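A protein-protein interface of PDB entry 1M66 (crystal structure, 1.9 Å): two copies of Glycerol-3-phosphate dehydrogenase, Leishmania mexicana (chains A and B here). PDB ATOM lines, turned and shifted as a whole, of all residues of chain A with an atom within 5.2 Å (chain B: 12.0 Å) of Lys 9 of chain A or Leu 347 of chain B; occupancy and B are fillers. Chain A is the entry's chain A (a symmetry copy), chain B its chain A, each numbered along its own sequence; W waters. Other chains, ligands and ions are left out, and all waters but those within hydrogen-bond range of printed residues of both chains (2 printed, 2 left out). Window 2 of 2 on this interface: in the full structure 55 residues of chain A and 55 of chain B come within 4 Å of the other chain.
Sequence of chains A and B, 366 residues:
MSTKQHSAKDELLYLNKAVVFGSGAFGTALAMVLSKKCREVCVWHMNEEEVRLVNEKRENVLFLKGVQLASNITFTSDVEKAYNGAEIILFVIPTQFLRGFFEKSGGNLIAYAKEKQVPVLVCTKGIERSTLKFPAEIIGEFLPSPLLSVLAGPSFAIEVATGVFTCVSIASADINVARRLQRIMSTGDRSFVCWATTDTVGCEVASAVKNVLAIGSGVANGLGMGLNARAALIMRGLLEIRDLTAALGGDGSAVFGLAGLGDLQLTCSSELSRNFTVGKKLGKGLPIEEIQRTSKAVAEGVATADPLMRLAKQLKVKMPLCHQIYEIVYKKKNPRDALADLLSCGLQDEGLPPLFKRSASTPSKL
Of the 13 printed residues of chain B, 5 touch a printed residue of chain A. Hydrophobic or aromatic side chains of chain B within 4 Å of the printed part of chain A: Leu 347. Of the 9 printed residues of chain A, 6 touch a printed residue of chain B. Among the printed residues, 10 pairs touch across the chains.
Lys 9 of chain A touches one residue of chain B. Leu 347 of chain B touches just these residues of chain A: Lys 9, Asp 10, Gln 182, Arg 183, Ser 186 and Arg 190. Of chain B, only Cys 345, Gly 346 and Leu 347 come within 4 Å of Asp 10 of chain A. No residue of chain B comes within 4 Å of Glu 11 of chain A. Gln 182 of chain A touches just these residues of chain B: Leu 347 (3.8 Å) and Gln 348 (2.7 Å). Arg 183 of chain A touches just one residue of chain B: Leu 347 (3.7 Å). No residue of chain B comes within 4 Å of Cys 194 of chain A. Of the printed residues of chain A, Leu 343 of chain B touches Arg 190 (3.2 Å). Printed residues of chain A within 4 Å of Cys 345 of chain B: Asp 10 (3.6 Å). Of the printed residues of chain A, Gly 346 of chain B touches Asp 10 (3.0 Å). Of the printed residues of chain B, Arg 190 of chain A touches Leu 343 and Leu 347. Gly 351 of chain B touches none of the printed residues of chain A. Asp 349 of chain B touches none of the printed residues of chain A.
Among the printed residues, merely in contact across the chains: Lys 9 of chain A with Leu 347 of chain B, Asp 10 of chain A with Cys 345 of chain B, Asp 10 of chain A with Gly 346 of chain B, Gln 182 of chain A with Leu 347 of chain B, Arg 183 of chain A with Leu 347 of chain B, Ser 186 of chain A with Leu 347 of chain B and Arg 190 of chain A with Leu 347 of chain B.
NE2 of Gln 182 of chain A lies within hydrogen-bond range of O of Cys 194 of chain A (2.8 Å). NH1 of Arg 183 of chain A lies close to O of Glu 11 of chain A, at 3.1 Å. The side-chain sulfur (SG) of Cys 345 of chain B lies within hydrogen-bond range of the backbone carbonyl oxygen (O) of Leu 342 of chain B (3.6 Å). The side-chain hydroxyl (OG) of Ser 186 of chain A sits at hydrogen-bond distance from the backbone NH (N) of Cys 194 of chain A (3.3 Å). O of Gln 182 of chain A sits at hydrogen-bond distance from OG of Ser 186 of chain A (2.7 Å).
No position is printed for both chains. Of the 10 pairs that touch across the chains among the printed residues, none has its exchanged pair printed and touching as well.
Water W2 lies within hydrogen-bond range of the backbone carbonyl oxygen of Cys 194 of chain A (2.7 Å), the backbone NH of Gln 348 of chain B (3.1 Å) and the side-chain amide nitrogen of Gln 182 of chain A (3.4 Å). Water W1 bridges O of Leu 343 of chain B (3.1 Å) and NE of Arg 190 of chain A (3.4 Å).
The backbone carbonyl oxygen (O) of Gln 348 of chain B sits at hydrogen-bond distance from the side-chain amide nitrogen (NE2) of Gln 182 of chain A. The backbone carbonyl oxygen of Leu 343 of chain B sits at hydrogen-bond distance from the guanidinium group of Arg 190 of chain A. The backbone NH (N) of Leu 347 of chain B sits at hydrogen-bond distance from the side-chain carboxylate (OD2) of Asp 10 of chain A (3.3 Å).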
ATOM      1  N   LYS A   9     -28.300 -31.686 -12.454  1.00  0.00           N
ATOM      2  CA  LYS A   9     -27.430 -32.894 -12.551  1.00  0.00           C
ATOM      3  C   LYS A   9     -26.700 -32.911 -13.892  1.00  0.00           C
ATOM      4  O   LYS A   9     -27.270 -32.543 -14.920  1.00  0.00           O
ATOM      5  CB  LYS A   9     -28.263 -34.168 -12.399  1.00  0.00           C
ATOM      6  CG  LYS A   9     -27.482 -35.361 -11.858  1.00  0.00           C
ATOM      7  CD  LYS A   9     -27.483 -35.367 -10.330  1.00  0.00           C
ATOM      8  CE  LYS A   9     -26.175 -35.908  -9.777  1.00  0.00           C
ATOM      9  NZ  LYS A   9     -25.031 -35.022 -10.152  1.00  0.00           N
ATOM     10  N   ASP A  10     -25.441 -33.341 -13.876  1.00  0.00           N
ATOM     11  CA  ASP A  10     -24.644 -33.423 -15.097  1.00  0.00           C
ATOM     12  C   ASP A  10     -24.861 -34.769 -15.794  1.00  0.00           C
ATOM     13  O   ASP A  10     -24.128 -35.137 -16.714  1.00  0.00           O
ATOM     14  CB  ASP A  10     -23.162 -33.221 -14.772  1.00  0.00           C
ATOM     15  CG  ASP A  10     -22.925 -32.040 -13.848  1.00  0.00           C
ATOM     16  OD1 ASP A  10     -23.620 -31.948 -12.812  1.00  0.00           O
ATOM     17  OD2 ASP A  10     -22.069 -31.155 -14.069  1.00  0.00           O
ATOM     18  N   GLU A  11     -25.884 -35.491 -15.348  1.00  0.00           N
ATOM     19  CA  GLU A  11     -26.214 -36.801 -15.884  1.00  0.00           C
ATOM     20  C   GLU A  11     -27.268 -36.675 -16.988  1.00  0.00           C
ATOM     21  O   GLU A  11     -28.337 -36.105 -16.768  1.00  0.00           O
ATOM     22  CB  GLU A  11     -26.735 -37.671 -14.742  1.00  0.00           C
ATOM     23  CG  GLU A  11     -26.890 -39.148 -15.046  1.00  0.00           C
ATOM     24  CD  GLU A  11     -27.233 -39.938 -13.798  1.00  0.00           C
ATOM     25  OE1 GLU A  11     -26.399 -39.973 -12.869  1.00  0.00           O
ATOM     26  OE2 GLU A  11     -28.346 -40.503 -13.732  1.00  0.00           O
ATOM     27  N   LEU A  12     -26.976 -37.228 -18.161  1.00  0.00           N
ATOM     28  CA  LEU A  12     -27.870 -37.098 -19.318  1.00  0.00           C
ATOM     29  C   LEU A  12     -29.223 -37.800 -19.178  1.00  0.00           C
ATOM     30  O   LEU A  12     -29.345 -38.787 -18.466  1.00  0.00           O
ATOM     31  CB  LEU A  12     -27.170 -37.567 -20.593  1.00  0.00           C
ATOM     32  CG  LEU A  12     -25.825 -36.894 -20.885  1.00  0.00           C
ATOM     33  CD1 LEU A  12     -25.247 -37.385 -22.222  1.00  0.00           C
ATOM     34  CD2 LEU A  12     -25.970 -35.371 -20.885  1.00  0.00           C
ATOM     35  N   GLN A 182     -31.342 -29.329 -21.228  1.00  0.00           N
ATOM     36  CA  GLN A 182     -29.906 -29.438 -21.431  1.00  0.00           C
ATOM     37  C   GLN A 182     -29.488 -30.905 -21.306  1.00  0.00           C
ATOM     38  O   GLN A 182     -28.609 -31.384 -22.023  1.00  0.00           O
ATOM     39  CB  GLN A 182     -29.239 -28.587 -20.346  1.00  0.00           C
ATOM     40  CG  GLN A 182     -27.771 -28.328 -20.442  1.00  0.00           C
ATOM     41  CD  GLN A 182     -27.302 -27.340 -19.373  1.00  0.00           C
ATOM     42  OE1 GLN A 182     -28.027 -27.049 -18.418  1.00  0.00           O
ATOM     43  NE2 GLN A 182     -26.101 -26.842 -19.527  1.00  0.00           N
ATOM     44  N   ARG A 183     -30.143 -31.618 -20.396  1.00  0.00           N
ATOM     45  CA  ARG A 183     -29.846 -33.030 -20.162  1.00  0.00           C
ATOM     46  C   ARG A 183     -30.382 -33.946 -21.251  1.00  0.00           C
ATOM     47  O   ARG A 183     -29.881 -35.048 -21.439  1.00  0.00           O
ATOM     48  CB  ARG A 183     -30.400 -33.465 -18.804  1.00  0.00           C
ATOM     49  CG  ARG A 183     -29.825 -32.687 -17.639  1.00  0.00           C
ATOM     50  CD  ARG A 183     -29.761 -33.481 -16.335  1.00  0.00           C
ATOM     51  NE  ARG A 183     -31.085 -33.824 -15.836  1.00  0.00           N
ATOM     52  CZ  ARG A 183     -31.340 -34.797 -14.975  1.00  0.00           C
ATOM     53  NH1 ARG A 183     -30.360 -35.563 -14.514  1.00  0.00           N
ATOM     54  NH2 ARG A 183     -32.590 -35.006 -14.574  1.00  0.00           N
ATOM     55  N   SER A 186     -28.168 -32.736 -24.928  1.00  0.00           N
ATOM     56  CA  SER A 186     -26.711 -32.914 -24.920  1.00  0.00           C
ATOM     57  C   SER A 186     -26.407 -34.393 -25.153  1.00  0.00           C
ATOM     58  O   SER A 186     -27.080 -35.259 -24.573  1.00  0.00           O
ATOM     59  CB  SER A 186     -26.135 -32.459 -23.593  1.00  0.00           C
ATOM     60  OG  SER A 186     -26.294 -31.048 -23.420  1.00  0.00           O
ATOM     61  N   ARG A 190     -20.434 -35.948 -26.278  1.00  0.00           N
ATOM     62  CA  ARG A 190     -20.082 -34.530 -26.070  1.00  0.00           C
ATOM     63  C   ARG A 190     -19.872 -33.765 -27.361  1.00  0.00           C
ATOM     64  O   ARG A 190     -19.167 -32.741 -27.383  1.00  0.00           O
ATOM     65  CB  ARG A 190     -18.866 -34.359 -25.156  1.00  0.00           C
ATOM     66  CG  ARG A 190     -18.973 -35.057 -23.790  1.00  0.00           C
ATOM     67  CD  ARG A 190     -20.012 -34.459 -22.844  1.00  0.00           C
ATOM     68  NE  ARG A 190     -19.524 -33.212 -22.246  1.00  0.00           N
ATOM     69  CZ  ARG A 190     -20.299 -32.188 -21.898  1.00  0.00           C
ATOM     70  NH1 ARG A 190     -21.620 -32.260 -22.072  1.00  0.00           N
ATOM     71  NH2 ARG A 190     -19.748 -31.095 -21.376  1.00  0.00           N
ATOM     72  N   CYS A 194     -24.978 -28.261 -24.655  1.00  0.00           N
ATOM     73  CA  CYS A 194     -25.953 -27.211 -24.409  1.00  0.00           C
ATOM     74  C   CYS A 194     -25.582 -26.463 -23.147  1.00  0.00           C
ATOM     75  O   CYS A 194     -25.095 -27.066 -22.184  1.00  0.00           O
ATOM     76  CB  CYS A 194     -27.336 -27.839 -24.258  1.00  0.00           C
ATOM     77  SG  CYS A 194     -27.868 -28.701 -25.748  1.00  0.00           S
ATOM     78  N   ARG B 236     -16.510 -18.770 -25.700  1.00  0.00           N
ATOM     79  CA  ARG B 236     -16.095 -19.192 -24.363  1.00  0.00           C
ATOM     80  C   ARG B 236     -14.765 -18.545 -24.029  1.00  0.00           C
ATOM     81  O   ARG B 236     -14.519 -18.113 -22.883  1.00  0.00           O
ATOM     82  CB  ARG B 236     -15.981 -20.724 -24.254  1.00  0.00           C
ATOM     83  CG  ARG B 236     -17.295 -21.494 -24.535  1.00  0.00           C
ATOM     84  CD  ARG B 236     -18.464 -21.073 -23.676  1.00  0.00           C
ATOM     85  NE  ARG B 236     -18.132 -21.145 -22.255  1.00  0.00           N
ATOM     86  CZ  ARG B 236     -18.897 -20.664 -21.280  1.00  0.00           C
ATOM     87  NH1 ARG B 236     -20.037 -20.051 -21.562  1.00  0.00           N
ATOM     88  NH2 ARG B 236     -18.531 -20.800 -20.017  1.00  0.00           N
ATOM     89  N   ALA B 340     -11.038 -33.469 -23.864  1.00  0.00           N
ATOM     90  CA  ALA B 340     -11.853 -34.283 -22.968  1.00  0.00           C
ATOM     91  C   ALA B 340     -11.838 -33.700 -21.568  1.00  0.00           C
ATOM     92  O   ALA B 340     -12.870 -33.634 -20.915  1.00  0.00           O
ATOM     93  CB  ALA B 340     -11.387 -35.750 -22.970  1.00  0.00           C
ATOM     94  N   ASP B 341     -10.672 -33.251 -21.120  1.00  0.00           N
ATOM     95  CA  ASP B 341     -10.565 -32.600 -19.827  1.00  0.00           C
ATOM     96  C   ASP B 341     -11.437 -31.344 -19.770  1.00  0.00           C
ATOM     97  O   ASP B 341     -12.102 -31.076 -18.770  1.00  0.00           O
ATOM     98  CB  ASP B 341      -9.106 -32.238 -19.544  1.00  0.00           C
ATOM     99  CG  ASP B 341      -8.305 -33.426 -19.046  1.00  0.00           C
ATOM    100  OD1 ASP B 341      -7.066 -33.394 -19.144  1.00  0.00           O
ATOM    101  OD2 ASP B 341      -8.846 -34.434 -18.544  1.00  0.00           O
ATOM    102  N   LEU B 342     -11.421 -30.576 -20.856  1.00  0.00           N
ATOM    103  CA  LEU B 342     -12.186 -29.348 -20.941  1.00  0.00           C
ATOM    104  C   LEU B 342     -13.665 -29.647 -20.846  1.00  0.00           C
ATOM    105  O   LEU B 342     -14.416 -28.898 -20.232  1.00  0.00           O
ATOM    106  CB  LEU B 342     -11.939 -28.673 -22.285  1.00  0.00           C
ATOM    107  CG  LEU B 342     -11.069 -27.436 -22.447  1.00  0.00           C
ATOM    108  CD1 LEU B 342     -11.385 -26.877 -23.813  1.00  0.00           C
ATOM    109  CD2 LEU B 342     -11.332 -26.394 -21.360  1.00  0.00           C
ATOM    110  N   LEU B 343     -14.078 -30.748 -21.470  1.00  0.00           N
ATOM    111  CA  LEU B 343     -15.486 -31.112 -21.517  1.00  0.00           C
ATOM    112  C   LEU B 343     -15.918 -31.990 -20.355  1.00  0.00           C
ATOM    113  O   LEU B 343     -17.013 -32.540 -20.381  1.00  0.00           O
ATOM    114  CB  LEU B 343     -15.808 -31.806 -22.841  1.00  0.00           C
ATOM    115  CG  LEU B 343     -15.551 -30.982 -24.106  1.00  0.00           C
ATOM    116  CD1 LEU B 343     -15.679 -31.846 -25.351  1.00  0.00           C
ATOM    117  CD2 LEU B 343     -16.493 -29.776 -24.181  1.00  0.00           C
ATOM    118  N   SER B 344     -15.070 -32.117 -19.340  1.00  0.00           N
ATOM    119  CA  SER B 344     -15.383 -32.970 -18.193  1.00  0.00           C
ATOM    120  C   SER B 344     -15.994 -32.195 -17.033  1.00  0.00           C
ATOM    121  O   SER B 344     -16.187 -32.738 -15.953  1.00  0.00           O
ATOM    122  CB  SER B 344     -14.113 -33.659 -17.692  1.00  0.00           C
ATOM    123  OG  SER B 344     -13.285 -32.717 -17.022  1.00  0.00           O
ATOM    124  N   CYS B 345     -16.305 -30.930 -17.260  1.00  0.00           N
ATOM    125  CA  CYS B 345     -16.823 -30.074 -16.203  1.00  0.00           C
ATOM    126  C   CYS B 345     -18.315 -30.264 -15.941  1.00  0.00           C
ATOM    127  O   CYS B 345     -18.851 -29.704 -14.996  1.00  0.00           O
ATOM    128  CB  CYS B 345     -16.537 -28.610 -16.543  1.00  0.00           C
ATOM    129  SG  CYS B 345     -17.249 -28.082 -18.128  1.00  0.00           S
ATOM    130  N   GLY B 346     -18.986 -31.047 -16.775  1.00  0.00           N
ATOM    131  CA  GLY B 346     -20.404 -31.282 -16.597  1.00  0.00           C
ATOM    132  C   GLY B 346     -21.245 -30.178 -17.210  1.00  0.00           C
ATOM    133  O   GLY B 346     -20.730 -29.171 -17.685  1.00  0.00           O
ATOM    134  N   LEU B 347     -22.553 -30.362 -17.187  1.00  0.00           N
ATOM    135  CA  LEU B 347     -23.463 -29.391 -17.766  1.00  0.00           C
ATOM    136  C   LEU B 347     -23.502 -28.115 -16.931  1.00  0.00           C
ATOM    137  O   LEU B 347     -23.553 -28.183 -15.703  1.00  0.00           O
ATOM    138  CB  LEU B 347     -24.860 -30.008 -17.852  1.00  0.00           C
ATOM    139  CG  LEU B 347     -24.941 -31.306 -18.651  1.00  0.00           C
ATOM    140  CD1 LEU B 347     -26.296 -31.972 -18.475  1.00  0.00           C
ATOM    141  CD2 LEU B 347     -24.689 -31.030 -20.096  1.00  0.00           C
ATOM    142  N   GLN B 348     -23.460 -26.950 -17.577  1.00  0.00           N
ATOM    143  CA  GLN B 348     -23.564 -25.702 -16.820  1.00  0.00           C
ATOM    144  C   GLN B 348     -24.344 -24.572 -17.471  1.00  0.00           C
ATOM    145  O   GLN B 348     -24.779 -24.671 -18.626  1.00  0.00           O
ATOM    146  CB  GLN B 348     -22.198 -25.187 -16.395  1.00  0.00           C
ATOM    147  CG  GLN B 348     -21.163 -25.213 -17.451  1.00  0.00           C
ATOM    148  CD  GLN B 348     -19.779 -25.215 -16.836  1.00  0.00           C
ATOM    149  OE1 GLN B 348     -18.884 -24.470 -17.265  1.00  0.00           O
ATOM    150  NE2 GLN B 348     -19.608 -26.031 -15.806  1.00  0.00           N
ATOM    151  N   ASP B 349     -24.532 -23.501 -16.699  1.00  0.00           N
ATOM    152  CA  ASP B 349     -25.196 -22.319 -17.214  1.00  0.00           C
ATOM    153  C   ASP B 349     -24.139 -21.585 -18.019  1.00  0.00           C
ATOM    154  O   ASP B 349     -22.936 -21.789 -17.812  1.00  0.00           O
ATOM    155  CB  ASP B 349     -25.708 -21.410 -16.090  1.00  0.00           C
ATOM    156  CG  ASP B 349     -26.746 -22.088 -15.188  1.00  0.00           C
ATOM    157  OD1 ASP B 349     -27.267 -23.189 -15.511  1.00  0.00           O
ATOM    158  OD2 ASP B 349     -27.105 -21.561 -14.112  1.00  0.00           O
ATOM    159  N   GLU B 350     -24.589 -20.703 -18.905  1.00  0.00           N
ATOM    160  CA  GLU B 350     -23.690 -19.972 -19.784  1.00  0.00           C
ATOM    161  C   GLU B 350     -22.701 -19.024 -19.088  1.00  0.00           C
ATOM    162  O   GLU B 350     -21.604 -18.792 -19.586  1.00  0.00           O
ATOM    163  CB  GLU B 350     -24.470 -19.261 -20.899  1.00  0.00           C
ATOM    164  CG  GLU B 350     -23.568 -18.753 -22.000  1.00  0.00           C
ATOM    165  CD  GLU B 350     -24.270 -18.523 -23.329  1.00  0.00           C
ATOM    166  OE1 GLU B 350     -25.471 -18.128 -23.371  1.00  0.00           O
ATOM    167  OE2 GLU B 350     -23.577 -18.686 -24.346  1.00  0.00           O
ATOM    168  N   GLY B 351     -23.048 -18.493 -17.929  1.00  0.00           N
ATOM    169  CA  GLY B 351     -22.070 -17.667 -17.214  1.00  0.00           C
ATOM    170  C   GLY B 351     -22.018 -16.191 -17.590  1.00  0.00           C
ATOM    171  O   GLY B 351     -21.014 -15.484 -17.355  1.00  0.00           O
HETATM  172  O   HOH W   1     -19.450 -33.912 -18.943  1.00  0.00           O
HETATM  173  O   HOH W   2     -22.933 -27.013 -20.629  1.00  0.00           O
